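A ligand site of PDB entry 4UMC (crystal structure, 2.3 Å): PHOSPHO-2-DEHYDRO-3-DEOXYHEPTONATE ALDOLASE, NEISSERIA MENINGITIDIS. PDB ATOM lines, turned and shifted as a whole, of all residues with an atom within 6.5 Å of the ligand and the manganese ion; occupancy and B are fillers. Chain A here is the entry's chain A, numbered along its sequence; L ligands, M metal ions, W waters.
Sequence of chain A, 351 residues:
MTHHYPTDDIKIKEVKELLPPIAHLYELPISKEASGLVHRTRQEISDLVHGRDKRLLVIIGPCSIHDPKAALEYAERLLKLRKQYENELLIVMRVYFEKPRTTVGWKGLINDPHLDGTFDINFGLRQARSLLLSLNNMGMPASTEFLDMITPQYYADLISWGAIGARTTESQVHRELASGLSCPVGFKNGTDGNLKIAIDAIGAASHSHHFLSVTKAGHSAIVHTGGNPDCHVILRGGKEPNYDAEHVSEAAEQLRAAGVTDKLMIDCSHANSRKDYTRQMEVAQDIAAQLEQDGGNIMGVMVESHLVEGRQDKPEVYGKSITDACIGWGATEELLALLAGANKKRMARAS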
ATOM      1  N   PRO A  62      39.831  27.806   9.606  1.00  0.00           N
ATOM      2  CA  PRO A  62      39.353  29.127   9.967  1.00  0.00           C
ATOM      3  C   PRO A  62      37.980  29.496   9.442  1.00  0.00           C
ATOM      4  O   PRO A  62      37.497  28.958   8.447  1.00  0.00           O
ATOM      5  CB  PRO A  62      40.381  30.059   9.344  1.00  0.00           C
ATOM      6  CG  PRO A  62      41.622  29.229   9.274  1.00  0.00           C
ATOM      7  CD  PRO A  62      41.136  27.840   8.943  1.00  0.00           C
ATOM      8  N   CYS A  63      37.331  30.412  10.128  1.00  0.00           N
ATOM      9  CA  CYS A  63      36.054  30.930   9.652  1.00  0.00           C
ATOM     10  C   CYS A  63      36.372  31.589   8.321  1.00  0.00           C
ATOM     11  O   CYS A  63      35.671  31.342   7.346  1.00  0.00           O
ATOM     12  CB  CYS A  63      35.454  31.915  10.643  1.00  0.00           C
ATOM     13  SG  CYS A  63      34.056  32.871  10.023  1.00  0.00           S
ATOM     14  N   SER A  64      37.447  32.393   8.281  1.00  0.00           N
ATOM     15  CA  SER A  64      37.881  33.058   7.068  1.00  0.00           C
ATOM     16  C   SER A  64      39.376  33.089   6.993  1.00  0.00           C
ATOM     17  O   SER A  64      40.021  33.186   8.008  1.00  0.00           O
ATOM     18  CB  SER A  64      37.402  34.505   7.050  1.00  0.00           C
ATOM     19  OG  SER A  64      37.818  35.198   8.218  1.00  0.00           O
ATOM     20  N   ARG A  94      39.007  24.132   5.717  1.00  0.00           N
ATOM     21  CA  ARG A  94      38.224  25.310   5.410  1.00  0.00           C
ATOM     22  C   ARG A  94      39.170  26.373   4.909  1.00  0.00           C
ATOM     23  O   ARG A  94      40.014  26.860   5.681  1.00  0.00           O
ATOM     24  CB  ARG A  94      37.516  25.893   6.629  1.00  0.00           C
ATOM     25  CG  ARG A  94      36.336  25.106   7.130  1.00  0.00           C
ATOM     26  CD  ARG A  94      35.710  25.763   8.346  1.00  0.00           C
ATOM     27  NE  ARG A  94      35.419  27.178   8.052  1.00  0.00           N
ATOM     28  CZ  ARG A  94      34.212  27.726   7.916  1.00  0.00           C
ATOM     29  NH1 ARG A  94      33.096  27.035   8.078  1.00  0.00           N
ATOM     30  NH2 ARG A  94      34.137  29.019   7.659  1.00  0.00           N
ATOM     31  N   TYR A  96      38.082  29.571   3.423  1.00  0.00           N
ATOM     32  CA  TYR A  96      36.980  30.472   3.016  1.00  0.00           C
ATOM     33  C   TYR A  96      37.458  31.858   2.591  1.00  0.00           C
ATOM     34  O   TYR A  96      38.019  32.610   3.395  1.00  0.00           O
ATOM     35  CB  TYR A  96      35.955  30.585   4.123  1.00  0.00           C
ATOM     36  CG  TYR A  96      34.983  29.414   4.226  1.00  0.00           C
ATOM     37  CD1 TYR A  96      35.416  28.076   4.141  1.00  0.00           C
ATOM     38  CD2 TYR A  96      33.623  29.632   4.429  1.00  0.00           C
ATOM     39  CE1 TYR A  96      34.523  27.005   4.285  1.00  0.00           C
ATOM     40  CE2 TYR A  96      32.734  28.569   4.568  1.00  0.00           C
ATOM     41  CZ  TYR A  96      33.189  27.269   4.501  1.00  0.00           C
ATOM     42  OH  TYR A  96      32.255  26.273   4.617  1.00  0.00           O
ATOM     43  N   LYS A  99      32.869  35.956   2.491  1.00  0.00           N
ATOM     44  CA  LYS A  99      32.087  35.985   3.741  1.00  0.00           C
ATOM     45  C   LYS A  99      30.771  36.806   3.568  1.00  0.00           C
ATOM     46  O   LYS A  99      30.802  37.958   3.127  1.00  0.00           O
ATOM     47  CB  LYS A  99      32.933  36.591   4.870  1.00  0.00           C
ATOM     48  CG  LYS A  99      34.244  35.888   5.159  1.00  0.00           C
ATOM     49  CD  LYS A  99      34.074  34.384   5.355  1.00  0.00           C
ATOM     50  CE  LYS A  99      33.235  34.064   6.558  1.00  0.00           C
ATOM     51  NZ  LYS A  99      33.134  32.595   6.762  1.00  0.00           N
ATOM     52  N   PRO A 100      29.628  36.227   3.945  1.00  0.00           N
ATOM     53  CA  PRO A 100      28.355  36.933   3.904  1.00  0.00           C
ATOM     54  C   PRO A 100      28.096  37.643   5.190  1.00  0.00           C
ATOM     55  O   PRO A 100      28.042  37.023   6.255  1.00  0.00           O
ATOM     56  CB  PRO A 100      27.348  35.810   3.723  1.00  0.00           C
ATOM     57  CG  PRO A 100      27.960  34.638   4.380  1.00  0.00           C
ATOM     58  CD  PRO A 100      29.446  34.783   4.196  1.00  0.00           C
ATOM     59  N   GLU A 145      33.224  28.468   0.841  1.00  0.00           N
ATOM     60  CA  GLU A 145      31.835  28.806   0.548  1.00  0.00           C
ATOM     61  C   GLU A 145      31.816  29.521  -0.770  1.00  0.00           C
ATOM     62  O   GLU A 145      32.590  30.444  -0.983  1.00  0.00           O
ATOM     63  CB  GLU A 145      31.189  29.719   1.614  1.00  0.00           C
ATOM     64  CG  GLU A 145      29.808  30.179   1.174  1.00  0.00           C
ATOM     65  CD  GLU A 145      29.050  31.063   2.127  1.00  0.00           C
ATOM     66  OE1 GLU A 145      29.392  31.091   3.329  1.00  0.00           O
ATOM     67  OE2 GLU A 145      28.077  31.716   1.645  1.00  0.00           O
ATOM     68  N   ILE A 164      27.248  26.175   0.223  1.00  0.00           N
ATOM     69  CA  ILE A 164      26.343  27.286  -0.035  1.00  0.00           C
ATOM     70  C   ILE A 164      25.752  27.667   1.285  1.00  0.00           C
ATOM     71  O   ILE A 164      25.149  26.831   1.990  1.00  0.00           O
ATOM     72  CB  ILE A 164      25.237  26.917  -0.993  1.00  0.00           C
ATOM     73  CG1 ILE A 164      25.818  26.503  -2.356  1.00  0.00           C
ATOM     74  CG2 ILE A 164      24.265  28.096  -1.142  1.00  0.00           C
ATOM     75  CD1 ILE A 164      26.488  27.604  -3.128  1.00  0.00           C
ATOM     76  N   GLY A 165      25.959  28.921   1.643  1.00  0.00           N
ATOM     77  CA  GLY A 165      25.654  29.384   3.001  1.00  0.00           C
ATOM     78  C   GLY A 165      24.186  29.430   3.358  1.00  0.00           C
ATOM     79  O   GLY A 165      23.319  29.402   2.507  1.00  0.00           O
ATOM     80  N   ALA A 166      23.937  29.569   4.648  1.00  0.00           N
ATOM     81  CA  ALA A 166      22.597  29.590   5.185  1.00  0.00           C
ATOM     82  C   ALA A 166      21.763  30.714   4.536  1.00  0.00           C
ATOM     83  O   ALA A 166      20.580  30.565   4.345  1.00  0.00           O
ATOM     84  CB  ALA A 166      22.628  29.770   6.692  1.00  0.00           C
ATOM     85  N   ARG A 167      22.426  31.810   4.219  1.00  0.00           N
ATOM     86  CA  ARG A 167      21.797  33.018   3.696  1.00  0.00           C
ATOM     87  C   ARG A 167      21.562  32.995   2.220  1.00  0.00           C
ATOM     88  O   ARG A 167      20.992  33.940   1.674  1.00  0.00           O
ATOM     89  CB  ARG A 167      22.662  34.236   4.019  1.00  0.00           C
ATOM     90  CG  ARG A 167      22.755  34.480   5.512  1.00  0.00           C
ATOM     91  CD  ARG A 167      23.749  35.577   5.895  1.00  0.00           C
ATOM     92  NE  ARG A 167      23.932  35.560   7.346  1.00  0.00           N
ATOM     93  CZ  ARG A 167      24.636  34.650   8.033  1.00  0.00           C
ATOM     94  NH1 ARG A 167      25.265  33.643   7.431  1.00  0.00           N
ATOM     95  NH2 ARG A 167      24.703  34.749   9.343  1.00  0.00           N
ATOM     96  N   LYS A 188      23.388  24.588   3.465  1.00  0.00           N
ATOM     97  CA  LYS A 188      23.089  24.810   4.858  1.00  0.00           C
ATOM     98  C   LYS A 188      21.648  25.174   5.060  1.00  0.00           C
ATOM     99  O   LYS A 188      21.072  25.814   4.237  1.00  0.00           O
ATOM    100  CB  LYS A 188      23.923  25.942   5.372  1.00  0.00           C
ATOM    101  CG  LYS A 188      25.398  25.572   5.398  1.00  0.00           C
ATOM    102  CD  LYS A 188      26.195  26.592   6.182  1.00  0.00           C
ATOM    103  CE  LYS A 188      27.118  25.895   7.147  1.00  0.00           C
ATOM    104  NZ  LYS A 188      27.852  26.927   7.903  1.00  0.00           N
ATOM    105  N   ASN A 189      21.068  24.736   6.170  1.00  0.00           N
ATOM    106  CA  ASN A 189      19.750  25.176   6.531  1.00  0.00           C
ATOM    107  C   ASN A 189      19.749  26.669   6.784  1.00  0.00           C
ATOM    108  O   ASN A 189      20.802  27.265   6.985  1.00  0.00           O
ATOM    109  CB  ASN A 189      19.180  24.369   7.716  1.00  0.00           C
ATOM    110  CG  ASN A 189      19.912  24.613   9.030  1.00  0.00           C
ATOM    111  OD1 ASN A 189      20.502  23.692   9.590  1.00  0.00           O
ATOM    112  ND2 ASN A 189      19.805  25.806   9.578  1.00  0.00           N
ATOM    113  N   THR A 191      18.946  30.587   8.310  1.00  0.00           N
ATOM    114  CA  THR A 191      19.461  31.171   9.534  1.00  0.00           C
ATOM    115  C   THR A 191      18.488  31.047  10.697  1.00  0.00           C
ATOM    116  O   THR A 191      18.916  31.103  11.841  1.00  0.00           O
ATOM    117  CB  THR A 191      19.892  32.634   9.356  1.00  0.00           C
ATOM    118  OG1 THR A 191      18.813  33.359   8.791  1.00  0.00           O
ATOM    119  CG2 THR A 191      21.074  32.738   8.444  1.00  0.00           C
ATOM    120  N   ARG A 236      23.200  23.465  10.616  1.00  0.00           N
ATOM    121  CA  ARG A 236      23.998  24.512  11.255  1.00  0.00           C
ATOM    122  C   ARG A 236      23.337  25.292  12.399  1.00  0.00           C
ATOM    123  O   ARG A 236      23.831  26.331  12.816  1.00  0.00           O
ATOM    124  CB  ARG A 236      24.556  25.486  10.200  1.00  0.00           C
ATOM    125  CG  ARG A 236      23.501  26.106   9.301  1.00  0.00           C
ATOM    126  CD  ARG A 236      22.828  27.288   9.981  1.00  0.00           C
ATOM    127  NE  ARG A 236      23.620  28.505   9.906  1.00  0.00           N
ATOM    128  CZ  ARG A 236      23.363  29.620  10.591  1.00  0.00           C
ATOM    129  NH1 ARG A 236      22.326  29.657  11.407  1.00  0.00           N
ATOM    130  NH2 ARG A 236      24.147  30.675  10.464  1.00  0.00           N
ATOM    131  N   ASP A 267      27.267  20.980  11.337  1.00  0.00           N
ATOM    132  CA  ASP A 267      28.182  22.055  11.663  1.00  0.00           C
ATOM    133  C   ASP A 267      28.229  22.205  13.195  1.00  0.00           C
ATOM    134  O   ASP A 267      27.209  22.418  13.816  1.00  0.00           O
ATOM    135  CB  ASP A 267      27.730  23.347  10.994  1.00  0.00           C
ATOM    136  CG  ASP A 267      28.699  24.515  11.181  1.00  0.00           C
ATOM    137  OD1 ASP A 267      29.776  24.382  11.805  1.00  0.00           O
ATOM    138  OD2 ASP A 267      28.369  25.603  10.655  1.00  0.00           O
ATOM    139  N   SER A 269      29.830  24.607  14.622  1.00  0.00           N
ATOM    140  CA  SER A 269      29.911  26.044  14.838  1.00  0.00           C
ATOM    141  C   SER A 269      28.602  26.794  14.591  1.00  0.00           C
ATOM    142  O   SER A 269      27.557  26.195  14.369  1.00  0.00           O
ATOM    143  CB  SER A 269      31.037  26.660  14.001  1.00  0.00           C
ATOM    144  OG  SER A 269      31.649  27.719  14.690  1.00  0.00           O
ATOM    145  N   HIS A 270      28.693  28.125  14.633  1.00  0.00           N
ATOM    146  CA  HIS A 270      27.572  28.993  14.283  1.00  0.00           C
ATOM    147  C   HIS A 270      26.349  28.796  15.173  1.00  0.00           C
ATOM    148  O   HIS A 270      26.459  28.862  16.392  1.00  0.00           O
ATOM    149  CB  HIS A 270      27.243  28.856  12.796  1.00  0.00           C
ATOM    150  CG  HIS A 270      28.416  29.138  11.907  1.00  0.00           C
ATOM    151  ND1 HIS A 270      29.098  28.143  11.237  1.00  0.00           N
ATOM    152  CD2 HIS A 270      29.044  30.288  11.593  1.00  0.00           C
ATOM    153  CE1 HIS A 270      30.085  28.675  10.533  1.00  0.00           C
ATOM    154  NE2 HIS A 270      30.067  29.976  10.740  1.00  0.00           N
ATOM    155  N   ALA A 271      25.174  28.595  14.580  1.00  0.00           N
ATOM    156  CA  ALA A 271      23.989  28.552  15.422  1.00  0.00           C
ATOM    157  C   ALA A 271      23.930  27.285  16.264  1.00  0.00           C
ATOM    158  O   ALA A 271      23.165  27.227  17.227  1.00  0.00           O
ATOM    159  CB  ALA A 271      22.705  28.720  14.575  1.00  0.00           C
ATOM    160  N   MET A 302      31.612  19.831  10.500  1.00  0.00           N
ATOM    161  CA  MET A 302      32.244  21.111  10.157  1.00  0.00           C
ATOM    162  C   MET A 302      32.703  21.722  11.472  1.00  0.00           C
ATOM    163  O   MET A 302      31.937  21.760  12.430  1.00  0.00           O
ATOM    164  CB  MET A 302      31.220  21.995   9.459  1.00  0.00           C
ATOM    165  CG  MET A 302      31.660  23.396   9.075  1.00  0.00           C
ATOM    166  SD  MET A 302      30.617  24.194   7.788  1.00  0.00           S
ATOM    167  CE  MET A 302      30.113  22.790   6.820  1.00  0.00           C
ATOM    168  N   GLU A 304      35.030  25.138  13.149  1.00  0.00           N
ATOM    169  CA  GLU A 304      35.784  26.390  13.000  1.00  0.00           C
ATOM    170  C   GLU A 304      36.985  26.398  13.963  1.00  0.00           C
ATOM    171  O   GLU A 304      36.843  26.492  15.190  1.00  0.00           O
ATOM    172  CB  GLU A 304      34.865  27.602  13.183  1.00  0.00           C
ATOM    173  CG  GLU A 304      34.032  27.893  11.927  1.00  0.00           C
ATOM    174  CD  GLU A 304      33.168  29.155  12.003  1.00  0.00           C
ATOM    175  OE1 GLU A 304      32.572  29.452  13.067  1.00  0.00           O
ATOM    176  OE2 GLU A 304      33.063  29.823  10.944  1.00  0.00           O
ATOM    177  N   THR A 323      37.067  37.121  11.865  1.00  0.00           N
ATOM    178  CA  THR A 323      35.637  36.822  11.720  1.00  0.00           C
ATOM    179  C   THR A 323      35.187  36.000  12.926  1.00  0.00           C
ATOM    180  O   THR A 323      35.538  36.315  14.053  1.00  0.00           O
ATOM    181  CB  THR A 323      35.309  36.122  10.394  1.00  0.00           C
ATOM    182  OG1 THR A 323      36.245  35.071  10.140  1.00  0.00           O
ATOM    183  CG2 THR A 323      35.367  37.117   9.253  1.00  0.00           C
ATOM    184  N   ASP A 324      34.379  34.965  12.704  1.00  0.00           N
ATOM    185  CA  ASP A 324      33.832  34.213  13.832  1.00  0.00           C
ATOM    186  C   ASP A 324      34.972  33.589  14.658  1.00  0.00           C
ATOM    187  O   ASP A 324      36.016  33.184  14.129  1.00  0.00           O
ATOM    188  CB  ASP A 324      32.859  33.097  13.367  1.00  0.00           C
ATOM    189  CG  ASP A 324      31.693  33.630  12.535  1.00  0.00           C
ATOM    190  OD1 ASP A 324      31.245  34.743  12.837  1.00  0.00           O
ATOM    191  OD2 ASP A 324      31.237  32.896  11.649  1.00  0.00           O
HETATM  192  C1  LIG L   1      30.812  30.500   7.728  1.00  0.00           C
HETATM  193  O1  LIG L   1      31.008  29.267   7.625  1.00  0.00           O
HETATM  194  O2  LIG L   1      31.642  31.336   8.198  1.00  0.00           O
HETATM  195  C2  LIG L   1      29.379  30.985   7.293  1.00  0.00           C
HETATM  196  C3  LIG L   1      29.103  32.488   7.546  1.00  0.00           C
HETATM  197  O3  LIG L   1      28.373  30.157   7.962  1.00  0.00           O
HETATM  198  P1  LIG L   1      26.709  30.215   7.723  1.00  0.00           P
HETATM  199  O4  LIG L   1      26.104  28.910   8.406  1.00  0.00           O
HETATM  200  O5  LIG L   1      26.229  31.473   8.657  1.00  0.00           O
HETATM  201  O6  LIG L   1      26.311  30.221   6.305  1.00  0.00           O
HETATM  202 MN    MN M   1      31.875  31.448  10.442  1.00  0.00          MN
HETATM  203  O   HOH W   1      28.437  28.963   4.543  1.00  0.00           O
HETATM  204  O   HOH W   2      25.289  32.251   4.922  1.00  0.00           O
HETATM  205  O   HOH W   3      30.134  35.346   7.539  1.00  0.00           O
HETATM  206  O   HOH W   4      29.792  27.302   5.750  1.00  0.00           O
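Residues that only touch the ligand: Gly 165 (3.5 Å), Tyr 96 (3.6 Å), Glu 145 (3.97 Å) and Pro 100 (3.99 Å). Hydrophobic or aromatic side chains that line the ligand: Tyr 96, Pro 100, Ala 166 and His 270.
Water W2 lies within hydrogen-bond range of O6 of the ligand, NH1 of Arg 167 and N of Ala 166. Water W4 lies within hydrogen-bond range of the side-chain hydroxyl of Tyr 96 (2.9 Å), the side-chain amino group of Lys 188 (2.9 Å) and an oxygen (O1) of the ligand (3.0 Å). Water W1 bridges the side-chain carboxylate of Glu 145 (2.6 Å) and an oxygen (O6) of the ligand (3.0 Å).
Along chain A the residues within 4 Å of the manganese ion span positions 63 to 324. The nearest printed residue that does not touch the manganese ion is Lys 99 (4.1 Å).
The side-chain amino group of Lys 99 lies close to an oxygen (O2) of the ligand, at 2.4 Å. An oxygen (O5) of the ligand lies within salt-bridge range of the guanidinium group (NH1) of Arg 167, at 2.7 Å. NZ of Lys 188 lies within salt-bridge range of O4 of the ligand (2.7 Å). NH2 of Arg 236 lies within salt-bridge range of O5 of the ligand (2.9 Å). O6 of the ligand sits at hydrogen-bond distance from N of Ala 166 (3.0 Å). NH1 of Arg 94 is in salt-bridge range of O1 of the ligand, at 3.1 Å.
OG of Ser 269 lies within hydrogen-bond range of OE1 of Glu 304 (2.5 Å). The side-chain carboxylate (OD2) of Asp 267 sits at hydrogen-bond distance from a ring nitrogen (ND1) of His 270 (2.7 Å). The backbone carbonyl oxygen of Cys 63 sits at hydrogen-bond distance from the guanidinium group of Arg 94, at 2.8 Å. SG of Cys 63 lies close to OG1 of Thr 323. The backbone NH of Lys 188 is in hydrogen-bond range of the backbone carbonyl oxygen of Ile 164 (3.2 Å). The backbone carbonyl oxygen of Arg 236 sits at hydrogen-bond distance from the backbone NH of Ala 271 (3.2 Å). SD of Met 302 sits at hydrogen-bond distance from NH1 of Arg 94, at 3.8 Å. The guanidinium group of Arg 94 is in hydrogen-bond range of the backbone carbonyl oxygen of Pro 62 (2.8 Å).
The side-chain carboxylate (OD2) of Asp 324 is bound to the manganese ion, 2.0 Å away. OE2 of Glu 304 binds the manganese ion (2.1 Å). The manganese ion is bound by O2 of the ligand (2.3 Å). The manganese ion is bound by a ring nitrogen (NE2) of His 270 (2.4 Å). The manganese ion is bound by SG of Cys 63 (2.6 Å). The manganese ion has five donor atoms within binding distance.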
